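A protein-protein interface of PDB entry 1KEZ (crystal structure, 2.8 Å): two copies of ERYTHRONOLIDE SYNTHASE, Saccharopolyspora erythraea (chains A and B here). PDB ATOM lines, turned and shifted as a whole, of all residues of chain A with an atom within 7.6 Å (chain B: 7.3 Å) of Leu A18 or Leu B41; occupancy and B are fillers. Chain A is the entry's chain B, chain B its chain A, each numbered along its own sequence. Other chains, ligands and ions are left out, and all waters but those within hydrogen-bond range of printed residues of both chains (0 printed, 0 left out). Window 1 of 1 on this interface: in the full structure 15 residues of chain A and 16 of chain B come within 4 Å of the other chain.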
ATOM      1  N   SER A  15     -25.516   5.542   1.899  1.00  0.00           N
ATOM      2  CA  SER A  15     -24.783   6.569   1.096  1.00  0.00           C
ATOM      3  C   SER A  15     -23.427   6.924   1.700  1.00  0.00           C
ATOM      4  O   SER A  15     -22.754   6.057   2.259  1.00  0.00           O
ATOM      5  CB  SER A  15     -25.665   7.820   0.888  1.00  0.00           C
ATOM      6  OG  SER A  15     -26.152   8.341   2.128  1.00  0.00           O
ATOM      7  N   SER A  16     -23.016   8.180   1.553  1.00  0.00           N
ATOM      8  CA  SER A  16     -21.733   8.640   2.091  1.00  0.00           C
ATOM      9  C   SER A  16     -21.758  10.106   2.550  1.00  0.00           C
ATOM     10  O   SER A  16     -22.773  10.793   2.407  1.00  0.00           O
ATOM     11  CB  SER A  16     -20.621   8.418   1.057  1.00  0.00           C
ATOM     12  OG  SER A  16     -20.966   9.031  -0.180  1.00  0.00           O
ATOM     13  N   ALA A  17     -20.648  10.571   3.122  1.00  0.00           N
ATOM     14  CA  ALA A  17     -20.549  11.945   3.608  1.00  0.00           C
ATOM     15  C   ALA A  17     -19.735  12.871   2.702  1.00  0.00           C
ATOM     16  O   ALA A  17     -20.002  14.074   2.645  1.00  0.00           O
ATOM     17  CB  ALA A  17     -19.976  11.967   5.035  1.00  0.00           C
ATOM     18  N   LEU A  18     -18.747  12.323   1.998  1.00  0.00           N
ATOM     19  CA  LEU A  18     -17.889  13.125   1.117  1.00  0.00           C
ATOM     20  C   LEU A  18     -18.486  13.449  -0.250  1.00  0.00           C
ATOM     21  O   LEU A  18     -18.205  14.508  -0.813  1.00  0.00           O
ATOM     22  CB  LEU A  18     -16.512  12.471   0.938  1.00  0.00           C
ATOM     23  CG  LEU A  18     -15.505  12.630   2.084  1.00  0.00           C
ATOM     24  CD1 LEU A  18     -16.053  12.016   3.351  1.00  0.00           C
ATOM     25  CD2 LEU A  18     -14.167  11.999   1.726  1.00  0.00           C
ATOM     26  N   ARG A  19     -19.321  12.562  -0.775  1.00  0.00           N
ATOM     27  CA  ARG A  19     -19.935  12.791  -2.076  1.00  0.00           C
ATOM     28  C   ARG A  19     -20.752  14.089  -2.089  1.00  0.00           C
ATOM     29  O   ARG A  19     -21.029  14.669  -3.149  1.00  0.00           O
ATOM     30  CB  ARG A  19     -20.810  11.586  -2.437  1.00  0.00           C
ATOM     31  CG  ARG A  19     -21.516  11.679  -3.789  1.00  0.00           C
ATOM     32  CD  ARG A  19     -22.611  10.636  -3.952  1.00  0.00           C
ATOM     33  NE  ARG A  19     -23.391  10.871  -5.171  1.00  0.00           N
ATOM     34  CZ  ARG A  19     -24.722  10.893  -5.234  1.00  0.00           C
ATOM     35  NH1 ARG A  19     -25.459  10.687  -4.143  1.00  0.00           N
ATOM     36  NH2 ARG A  19     -25.323  11.167  -6.387  1.00  0.00           N
ATOM     37  N   ASP A  20     -21.112  14.541  -0.891  1.00  0.00           N
ATOM     38  CA  ASP A  20     -21.906  15.755  -0.692  1.00  0.00           C
ATOM     39  C   ASP A  20     -21.113  17.030  -0.932  1.00  0.00           C
ATOM     40  O   ASP A  20     -21.569  17.917  -1.648  1.00  0.00           O
ATOM     41  CB  ASP A  20     -22.482  15.777   0.729  1.00  0.00           C
ATOM     42  CG  ASP A  20     -23.447  16.919   0.950  1.00  0.00           C
ATOM     43  OD1 ASP A  20     -23.099  17.902   1.641  1.00  0.00           O
ATOM     44  OD2 ASP A  20     -24.567  16.834   0.414  1.00  0.00           O
ATOM     45  N   GLY A  21     -19.943  17.131  -0.306  1.00  0.00           N
ATOM     46  CA  GLY A  21     -19.096  18.300  -0.481  1.00  0.00           C
ATOM     47  C   GLY A  21     -18.486  18.414  -1.867  1.00  0.00           C
ATOM     48  O   GLY A  21     -18.127  19.508  -2.307  1.00  0.00           O
ATOM     49  N   TYR A  22     -18.382  17.276  -2.548  1.00  0.00           N
ATOM     50  CA  TYR A  22     -17.815  17.176  -3.892  1.00  0.00           C
ATOM     51  C   TYR A  22     -18.525  18.110  -4.890  1.00  0.00           C
ATOM     52  O   TYR A  22     -17.885  18.849  -5.643  1.00  0.00           O
ATOM     53  CB  TYR A  22     -17.917  15.716  -4.352  1.00  0.00           C
ATOM     54  CG  TYR A  22     -17.205  15.387  -5.646  1.00  0.00           C
ATOM     55  CD1 TYR A  22     -15.826  15.166  -5.675  1.00  0.00           C
ATOM     56  CD2 TYR A  22     -17.907  15.303  -6.846  1.00  0.00           C
ATOM     57  CE1 TYR A  22     -15.171  14.870  -6.867  1.00  0.00           C
ATOM     58  CE2 TYR A  22     -17.261  15.011  -8.042  1.00  0.00           C
ATOM     59  CZ  TYR A  22     -15.897  14.797  -8.047  1.00  0.00           C
ATOM     60  OH  TYR A  22     -15.276  14.514  -9.243  1.00  0.00           O
ATOM     61  N   ARG A  23     -19.852  18.103  -4.851  1.00  0.00           N
ATOM     62  CA  ARG A  23     -20.650  18.934  -5.739  1.00  0.00           C
ATOM     63  C   ARG A  23     -20.930  20.336  -5.173  1.00  0.00           C
ATOM     64  O   ARG A  23     -21.218  21.262  -5.938  1.00  0.00           O
ATOM     65  CB  ARG A  23     -21.952  18.211  -6.099  1.00  0.00           C
ATOM     66  CG  ARG A  23     -22.566  18.697  -7.385  1.00  0.00           C
ATOM     67  CD  ARG A  23     -23.734  17.830  -7.832  1.00  0.00           C
ATOM     68  NE  ARG A  23     -24.902  17.934  -6.960  1.00  0.00           N
ATOM     69  CZ  ARG A  23     -26.152  17.909  -7.408  1.00  0.00           C
ATOM     70  NH1 ARG A  23     -26.384  17.785  -8.707  1.00  0.00           N
ATOM     71  NH2 ARG A  23     -27.169  18.021  -6.567  1.00  0.00           N
ATOM     72  N   GLN A  24     -20.864  20.493  -3.849  1.00  0.00           N
ATOM     73  CA  GLN A  24     -21.108  21.798  -3.219  1.00  0.00           C
ATOM     74  C   GLN A  24     -19.885  22.709  -3.354  1.00  0.00           C
ATOM     75  O   GLN A  24     -19.949  23.911  -3.081  1.00  0.00           O
ATOM     76  CB  GLN A  24     -21.499  21.640  -1.741  1.00  0.00           C
ATOM     77  CG  GLN A  24     -21.904  22.955  -1.019  1.00  0.00           C
ATOM     78  CD  GLN A  24     -23.236  23.546  -1.486  1.00  0.00           C
ATOM     79  OE1 GLN A  24     -23.989  22.918  -2.235  1.00  0.00           O
ATOM     80  NE2 GLN A  24     -23.533  24.763  -1.028  1.00  0.00           N
ATOM     81  N   TYR A  34     -10.208  22.391  -1.016  1.00  0.00           N
ATOM     82  CA  TYR A  34     -10.700  21.046  -0.721  1.00  0.00           C
ATOM     83  C   TYR A  34      -9.625  19.964  -0.872  1.00  0.00           C
ATOM     84  O   TYR A  34      -9.604  18.985  -0.125  1.00  0.00           O
ATOM     85  CB  TYR A  34     -11.882  20.713  -1.638  1.00  0.00           C
ATOM     86  CG  TYR A  34     -12.851  19.677  -1.088  1.00  0.00           C
ATOM     87  CD1 TYR A  34     -12.700  19.172   0.198  1.00  0.00           C
ATOM     88  CD2 TYR A  34     -13.950  19.249  -1.836  1.00  0.00           C
ATOM     89  CE1 TYR A  34     -13.610  18.281   0.733  1.00  0.00           C
ATOM     90  CE2 TYR A  34     -14.878  18.353  -1.309  1.00  0.00           C
ATOM     91  CZ  TYR A  34     -14.699  17.875  -0.020  1.00  0.00           C
ATOM     92  OH  TYR A  34     -15.617  17.013   0.533  1.00  0.00           O
ATOM     93  N   LEU A  37      -7.160  19.344   1.908  1.00  0.00           N
ATOM     94  CA  LEU A  37      -7.814  18.587   2.969  1.00  0.00           C
ATOM     95  C   LEU A  37      -7.614  17.069   2.766  1.00  0.00           C
ATOM     96  O   LEU A  37      -7.099  16.390   3.657  1.00  0.00           O
ATOM     97  CB  LEU A  37      -9.310  18.947   2.988  1.00  0.00           C
ATOM     98  CG  LEU A  37     -10.054  19.114   4.317  1.00  0.00           C
ATOM     99  CD1 LEU A  37     -10.385  17.769   4.900  1.00  0.00           C
ATOM    100  CD2 LEU A  37      -9.231  19.948   5.290  1.00  0.00           C
ATOM    101  N   LEU A  38      -7.992  16.575   1.585  1.00  0.00           N
ATOM    102  CA  LEU A  38      -7.890  15.166   1.213  1.00  0.00           C
ATOM    103  C   LEU A  38      -6.560  14.486   1.567  1.00  0.00           C
ATOM    104  O   LEU A  38      -6.512  13.634   2.466  1.00  0.00           O
ATOM    105  CB  LEU A  38      -8.219  14.996  -0.275  1.00  0.00           C
ATOM    106  CG  LEU A  38      -9.656  15.273  -0.734  1.00  0.00           C
ATOM    107  CD1 LEU A  38      -9.861  14.686  -2.123  1.00  0.00           C
ATOM    108  CD2 LEU A  38     -10.674  14.659   0.233  1.00  0.00           C
ATOM    109  N   LEU A  41      -5.301  12.910   4.981  1.00  0.00           N
ATOM    110  CA  LEU A  41      -5.637  11.602   5.535  1.00  0.00           C
ATOM    111  C   LEU A  41      -4.785  10.473   4.978  1.00  0.00           C
ATOM    112  O   LEU A  41      -4.965   9.321   5.360  1.00  0.00           O
ATOM    113  CB  LEU A  41      -7.108  11.275   5.261  1.00  0.00           C
ATOM    114  CG  LEU A  41      -8.179  12.255   5.741  1.00  0.00           C
ATOM    115  CD1 LEU A  41      -9.526  11.900   5.133  1.00  0.00           C
ATOM    116  CD2 LEU A  41      -8.264  12.275   7.255  1.00  0.00           C
ATOM    117  N   MET A 198     -20.440   5.715  -6.718  1.00  0.00           N
ATOM    118  CA  MET A 198     -19.277   6.353  -6.130  1.00  0.00           C
ATOM    119  C   MET A 198     -19.274   6.275  -4.595  1.00  0.00           C
ATOM    120  O   MET A 198     -19.688   7.221  -3.912  1.00  0.00           O
ATOM    121  CB  MET A 198     -19.179   7.802  -6.643  1.00  0.00           C
ATOM    122  CG  MET A 198     -19.165   7.916  -8.187  1.00  0.00           C
ATOM    123  SD  MET A 198     -19.186   9.600  -8.885  1.00  0.00           S
ATOM    124  CE  MET A 198     -17.506   9.779  -9.495  1.00  0.00           C
ATOM    125  N   ASP A 200     -17.427   5.267  -0.636  1.00  0.00           N
ATOM    126  CA  ASP A 200     -16.275   5.666   0.182  1.00  0.00           C
ATOM    127  C   ASP A 200     -14.894   5.010  -0.018  1.00  0.00           C
ATOM    128  O   ASP A 200     -14.185   4.732   0.955  1.00  0.00           O
ATOM    129  CB  ASP A 200     -16.675   5.609   1.667  1.00  0.00           C
ATOM    130  CG  ASP A 200     -17.081   4.216   2.114  1.00  0.00           C
ATOM    131  OD1 ASP A 200     -16.259   3.540   2.760  1.00  0.00           O
ATOM    132  OD2 ASP A 200     -18.222   3.794   1.834  1.00  0.00           O
ATOM    133  N   LEU A 203     -12.659   7.826  -3.896  1.00  0.00           N
ATOM    134  CA  LEU A 203     -12.339   9.243  -3.749  1.00  0.00           C
ATOM    135  C   LEU A 203     -10.978   9.527  -3.108  1.00  0.00           C
ATOM    136  O   LEU A 203     -10.235  10.392  -3.571  1.00  0.00           O
ATOM    137  CB  LEU A 203     -13.434   9.951  -2.955  1.00  0.00           C
ATOM    138  CG  LEU A 203     -14.501  10.591  -3.835  1.00  0.00           C
ATOM    139  CD1 LEU A 203     -15.565  11.215  -2.968  1.00  0.00           C
ATOM    140  CD2 LEU A 203     -13.876  11.650  -4.737  1.00  0.00           C
ATOM    141  N   THR A 204     -10.673   8.802  -2.033  1.00  0.00           N
ATOM    142  CA  THR A 204      -9.419   8.951  -1.294  1.00  0.00           C
ATOM    143  C   THR A 204      -8.161   8.651  -2.107  1.00  0.00           C
ATOM    144  O   THR A 204      -7.039   8.846  -1.626  1.00  0.00           O
ATOM    145  CB  THR A 204      -9.387   8.063  -0.024  1.00  0.00           C
ATOM    146  OG1 THR A 204      -9.744   6.715  -0.349  1.00  0.00           O
ATOM    147  CG2 THR A 204     -10.337   8.577   1.034  1.00  0.00           C
ATOM    148  N   LEU B  18     -13.508   4.652   6.295  1.00  0.00           N
ATOM    149  CA  LEU B  18     -13.203   5.610   7.340  1.00  0.00           C
ATOM    150  C   LEU B  18     -13.198   4.938   8.725  1.00  0.00           C
ATOM    151  O   LEU B  18     -13.002   5.592   9.756  1.00  0.00           O
ATOM    152  CB  LEU B  18     -14.220   6.757   7.265  1.00  0.00           C
ATOM    153  CG  LEU B  18     -13.686   8.178   7.491  1.00  0.00           C
ATOM    154  CD1 LEU B  18     -12.620   8.528   6.437  1.00  0.00           C
ATOM    155  CD2 LEU B  18     -14.836   9.184   7.486  1.00  0.00           C
ATOM    156  N   LEU B  35      -7.713  15.445  12.860  1.00  0.00           N
ATOM    157  CA  LEU B  35      -8.905  16.225  13.158  1.00  0.00           C
ATOM    158  C   LEU B  35      -9.017  17.515  12.354  1.00  0.00           C
ATOM    159  O   LEU B  35     -10.124  17.968  12.056  1.00  0.00           O
ATOM    160  CB  LEU B  35      -8.991  16.510  14.661  1.00  0.00           C
ATOM    161  CG  LEU B  35      -9.098  15.345  15.659  1.00  0.00           C
ATOM    162  CD1 LEU B  35      -9.082  15.913  17.066  1.00  0.00           C
ATOM    163  CD2 LEU B  35     -10.365  14.525  15.443  1.00  0.00           C
ATOM    164  N   ASP B  36      -7.876  18.112  12.019  1.00  0.00           N
ATOM    165  CA  ASP B  36      -7.861  19.347  11.235  1.00  0.00           C
ATOM    166  C   ASP B  36      -8.661  19.120   9.944  1.00  0.00           C
ATOM    167  O   ASP B  36      -9.340  20.026   9.455  1.00  0.00           O
ATOM    168  CB  ASP B  36      -6.409  19.733  10.910  1.00  0.00           C
ATOM    169  CG  ASP B  36      -6.264  21.173  10.456  1.00  0.00           C
ATOM    170  OD1 ASP B  36      -6.184  22.077  11.319  1.00  0.00           O
ATOM    171  OD2 ASP B  36      -6.198  21.410   9.231  1.00  0.00           O
ATOM    172  N   LEU B  37      -8.604  17.891   9.428  1.00  0.00           N
ATOM    173  CA  LEU B  37      -9.318  17.518   8.206  1.00  0.00           C
ATOM    174  C   LEU B  37     -10.807  17.197   8.393  1.00  0.00           C
ATOM    175  O   LEU B  37     -11.624  17.589   7.565  1.00  0.00           O
ATOM    176  CB  LEU B  37      -8.631  16.342   7.490  1.00  0.00           C
ATOM    177  CG  LEU B  37      -7.185  16.438   6.986  1.00  0.00           C
ATOM    178  CD1 LEU B  37      -6.732  17.884   6.828  1.00  0.00           C
ATOM    179  CD2 LEU B  37      -6.286  15.710   7.951  1.00  0.00           C
ATOM    180  N   LEU B  38     -11.160  16.488   9.464  1.00  0.00           N
ATOM    181  CA  LEU B  38     -12.565  16.137   9.705  1.00  0.00           C
ATOM    182  C   LEU B  38     -13.456  17.382   9.676  1.00  0.00           C
ATOM    183  O   LEU B  38     -14.611  17.326   9.251  1.00  0.00           O
ATOM    184  CB  LEU B  38     -12.736  15.402  11.044  1.00  0.00           C
ATOM    185  CG  LEU B  38     -11.799  14.238  11.394  1.00  0.00           C
ATOM    186  CD1 LEU B  38     -12.273  13.519  12.653  1.00  0.00           C
ATOM    187  CD2 LEU B  38     -11.712  13.260  10.238  1.00  0.00           C
ATOM    188  N   ALA B  39     -12.906  18.504  10.130  1.00  0.00           N
ATOM    189  CA  ALA B  39     -13.625  19.771  10.155  1.00  0.00           C
ATOM    190  C   ALA B  39     -13.587  20.444   8.783  1.00  0.00           C
ATOM    191  O   ALA B  39     -14.375  21.346   8.497  1.00  0.00           O
ATOM    192  CB  ALA B  39     -13.020  20.686  11.204  1.00  0.00           C
ATOM    193  N   GLY B  40     -12.625  20.044   7.957  1.00  0.00           N
ATOM    194  CA  GLY B  40     -12.509  20.609   6.625  1.00  0.00           C
ATOM    195  C   GLY B  40     -13.573  20.034   5.712  1.00  0.00           C
ATOM    196  O   GLY B  40     -14.088  20.713   4.820  1.00  0.00           O
ATOM    197  N   LEU B  41     -13.900  18.769   5.943  1.00  0.00           N
ATOM    198  CA  LEU B  41     -14.900  18.074   5.147  1.00  0.00           C
ATOM    199  C   LEU B  41     -16.314  18.480   5.524  1.00  0.00           C
ATOM    200  O   LEU B  41     -17.213  18.466   4.682  1.00  0.00           O
ATOM    201  CB  LEU B  41     -14.762  16.555   5.323  1.00  0.00           C
ATOM    202  CG  LEU B  41     -13.542  15.870   4.682  1.00  0.00           C
ATOM    203  CD1 LEU B  41     -13.381  14.437   5.191  1.00  0.00           C
ATOM    204  CD2 LEU B  41     -13.656  15.903   3.162  1.00  0.00           C
ATOM    205  N   SER B  42     -16.514  18.790   6.802  1.00  0.00           N
ATOM    206  CA  SER B  42     -17.828  19.171   7.319  1.00  0.00           C
ATOM    207  C   SER B  42     -18.258  20.558   6.871  1.00  0.00           C
ATOM    208  O   SER B  42     -19.453  20.845   6.804  1.00  0.00           O
ATOM    209  CB  SER B  42     -17.850  19.092   8.850  1.00  0.00           C
ATOM    210  OG  SER B  42     -17.097  20.132   9.452  1.00  0.00           O
ATOM    211  N   ASP B  43     -17.280  21.416   6.582  1.00  0.00           N
ATOM    212  CA  ASP B  43     -17.548  22.780   6.135  1.00  0.00           C
ATOM    213  C   ASP B  43     -18.315  22.772   4.807  1.00  0.00           C
ATOM    214  O   ASP B  43     -18.978  23.747   4.448  1.00  0.00           O
ATOM    215  CB  ASP B  43     -16.227  23.550   5.987  1.00  0.00           C
ATOM    216  CG  ASP B  43     -16.419  25.063   5.970  1.00  0.00           C
ATOM    217  OD1 ASP B  43     -15.445  25.791   5.668  1.00  0.00           O
ATOM    218  OD2 ASP B  43     -17.532  25.540   6.276  1.00  0.00           O
ATOM    219  N   PHE B  44     -18.249  21.645   4.103  1.00  0.00           N
ATOM    220  CA  PHE B  44     -18.920  21.491   2.817  1.00  0.00           C
ATOM    221  C   PHE B  44     -20.364  21.019   2.919  1.00  0.00           C
ATOM    222  O   PHE B  44     -21.191  21.379   2.082  1.00  0.00           O
ATOM    223  CB  PHE B  44     -18.109  20.581   1.897  1.00  0.00           C
ATOM    224  CG  PHE B  44     -16.859  21.228   1.376  1.00  0.00           C
ATOM    225  CD1 PHE B  44     -16.749  21.591   0.037  1.00  0.00           C
ATOM    226  CD2 PHE B  44     -15.805  21.520   2.237  1.00  0.00           C
ATOM    227  CE1 PHE B  44     -15.612  22.236  -0.434  1.00  0.00           C
ATOM    228  CE2 PHE B  44     -14.666  22.164   1.773  1.00  0.00           C
ATOM    229  CZ  PHE B  44     -14.567  22.524   0.438  1.00  0.00           C
ATOM    230  N   ARG B  45     -20.663  20.209   3.932  1.00  0.00           N
ATOM    231  CA  ARG B  45     -22.023  19.702   4.152  1.00  0.00           C
ATOM    232  C   ARG B  45     -22.970  20.870   4.416  1.00  0.00           C
ATOM    233  O   ARG B  45     -22.529  21.957   4.808  1.00  0.00           O
ATOM    234  CB  ARG B  45     -22.052  18.788   5.380  1.00  0.00           C
ATOM    235  CG  ARG B  45     -21.304  17.477   5.237  1.00  0.00           C
ATOM    236  CD  ARG B  45     -22.178  16.406   4.610  1.00  0.00           C
ATOM    237  NE  ARG B  45     -23.441  16.237   5.328  1.00  0.00           N
ATOM    238  CZ  ARG B  45     -23.554  15.733   6.554  1.00  0.00           C
ATOM    239  NH1 ARG B  45     -22.479  15.337   7.221  1.00  0.00           N
ATOM    240  NH2 ARG B  45     -24.748  15.639   7.119  1.00  0.00           N
ATOM    241  N   HIS B  47     -25.326  23.344   6.249  1.00  0.00           N
ATOM    242  CA  HIS B  47     -25.223  23.828   7.622  1.00  0.00           C
ATOM    243  C   HIS B  47     -26.463  24.565   8.118  1.00  0.00           C
ATOM    244  O   HIS B  47     -27.309  24.973   7.328  1.00  0.00           O
ATOM    245  CB  HIS B  47     -24.044  24.797   7.734  1.00  0.00           C
ATOM    246  CG  HIS B  47     -22.700  24.154   7.616  1.00  0.00           C
ATOM    247  ND1 HIS B  47     -21.681  24.702   6.868  1.00  0.00           N
ATOM    248  CD2 HIS B  47     -22.182  23.049   8.206  1.00  0.00           C
ATOM    249  CE1 HIS B  47     -20.591  23.968   7.008  1.00  0.00           C
ATOM    250  NE2 HIS B  47     -20.870  22.960   7.815  1.00  0.00           N
ATOM    251  N   LEU B 112     -25.000  20.192   9.904  1.00  0.00           N
ATOM    252  CA  LEU B 112     -24.000  20.580  10.915  1.00  0.00           C
ATOM    253  C   LEU B 112     -24.006  22.104  11.155  1.00  0.00           C
ATOM    254  O   LEU B 112     -24.243  22.885  10.235  1.00  0.00           O
ATOM    255  CB  LEU B 112     -22.608  20.137  10.463  1.00  0.00           C
ATOM    256  CG  LEU B 112     -22.499  18.753   9.818  1.00  0.00           C
ATOM    257  CD1 LEU B 112     -21.115  18.554   9.241  1.00  0.00           C
ATOM    258  CD2 LEU B 112     -22.831  17.647  10.806  1.00  0.00           C
ATOM    259  N   ASP B 200     -20.171   6.482   8.618  1.00  0.00           N
ATOM    260  CA  ASP B 200     -19.386   7.566   8.030  1.00  0.00           C
ATOM    261  C   ASP B 200     -19.812   8.974   8.441  1.00  0.00           C
ATOM    262  O   ASP B 200     -18.960   9.836   8.656  1.00  0.00           O
ATOM    263  CB  ASP B 200     -19.373   7.440   6.501  1.00  0.00           C
ATOM    264  CG  ASP B 200     -20.765   7.282   5.913  1.00  0.00           C
ATOM    265  OD1 ASP B 200     -21.344   8.296   5.476  1.00  0.00           O
ATOM    266  OD2 ASP B 200     -21.286   6.143   5.882  1.00  0.00           O
ATOM    267  N   THR B 201     -21.120   9.202   8.559  1.00  0.00           N
ATOM    268  CA  THR B 201     -21.632  10.520   8.938  1.00  0.00           C
ATOM    269  C   THR B 201     -21.425  10.902  10.405  1.00  0.00           C
ATOM    270  O   THR B 201     -21.704  12.033  10.804  1.00  0.00           O
ATOM    271  CB  THR B 201     -23.123  10.706   8.540  1.00  0.00           C
ATOM    272  OG1 THR B 201     -23.892   9.569   8.955  1.00  0.00           O
ATOM    273  CG2 THR B 201     -23.255  10.878   7.034  1.00  0.00           C
ATOM    274  N   THR B 204     -17.482  12.350  10.637  1.00  0.00           N
ATOM    275  CA  THR B 204     -17.353  13.672  10.035  1.00  0.00           C
ATOM    276  C   THR B 204     -17.897  14.746  10.979  1.00  0.00           C
ATOM    277  O   THR B 204     -17.337  15.849  11.082  1.00  0.00           O
ATOM    278  CB  THR B 204     -18.058  13.741   8.654  1.00  0.00           C
ATOM    279  OG1 THR B 204     -19.440  13.379   8.775  1.00  0.00           O
ATOM    280  CG2 THR B 204     -17.382  12.791   7.668  1.00  0.00           C
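Hydrophobic or aromatic side chains of chain A that line the printed part of chain B: Ala A17, Leu A18, Tyr A34 and Leu A37.
Among the printed residues, no Asp or Glu carboxylate lies within 4 Å of a Lys or Arg side-chain nitrogen of the other chain.
O of Ser A15 touches OD2 of Asp B200 (3.9 Å).
Asp B200 touches Ser A16 (OD1 to CA, 3.4 Å).
Ala A17 touches Arg B45 (O to CD, 3.7 Å).
CG2 of Thr B201 touches CB of Ala A17, 3.99 Å away.
Thr B204 touches Ala A17.
Leu B41 touches Leu A18 (CD2 to CG, 3.9 Å).
Asp A20 touches Arg B45 (OD1 to CA, 3.3 Å).
Leu B41 touches Tyr A34 (CD2 to CE1, 3.4 Å).
CG of Tyr A34 touches CZ of Phe B44, at 3.7 Å.
Leu A37 touches Leu B37.
Of the printed residues of chain B, Ser A15 touches Asp B200.
Leu A18 touches just one residue of chain B: Leu B41.
Printed residues of chain B within 4 Å of Asp A20: Phe B44 (3.99 Å) and Arg B45 (3.3 Å).
Printed residues of chain B within 4 Å of Gly A21: Phe B44.
Of chain A, only Leu A37 comes within 4 Å of Gly B40.
Leu B41 touches three residues of chain A.
Of the printed residues of chain A, Asp B200 touches Ser A15 (3.9 Å), Ser A16 (3.4 Å) and Ala A17 (3.3 Å).
Of the printed residues of chain A, Thr B201 touches Ala A17 (3.99 Å).
The nearest printed residue of chain A that does not touch Leu B37 is Leu A41 (4.02 Å).
OD1 of Asp B200 sits at hydrogen-bond distance from N of Ala A17.
O of Thr B201 is in hydrogen-bond range of OG1 of Thr B204 (3.3 Å).
Leu A18 touches Leu B41, but with the chains exchanged Leu A41 does not touch Leu B18 (4.8 Å).
Leu B37 touches its own counterpart, Leu A37.
Leu A37 touches Leu B41, but with the chains exchanged Leu A41 does not touch Leu B37 (4.02 Å).
Of the 16 pairs that touch across the chains among the printed residues, 1 has its exchanged pair printed and touching as well.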
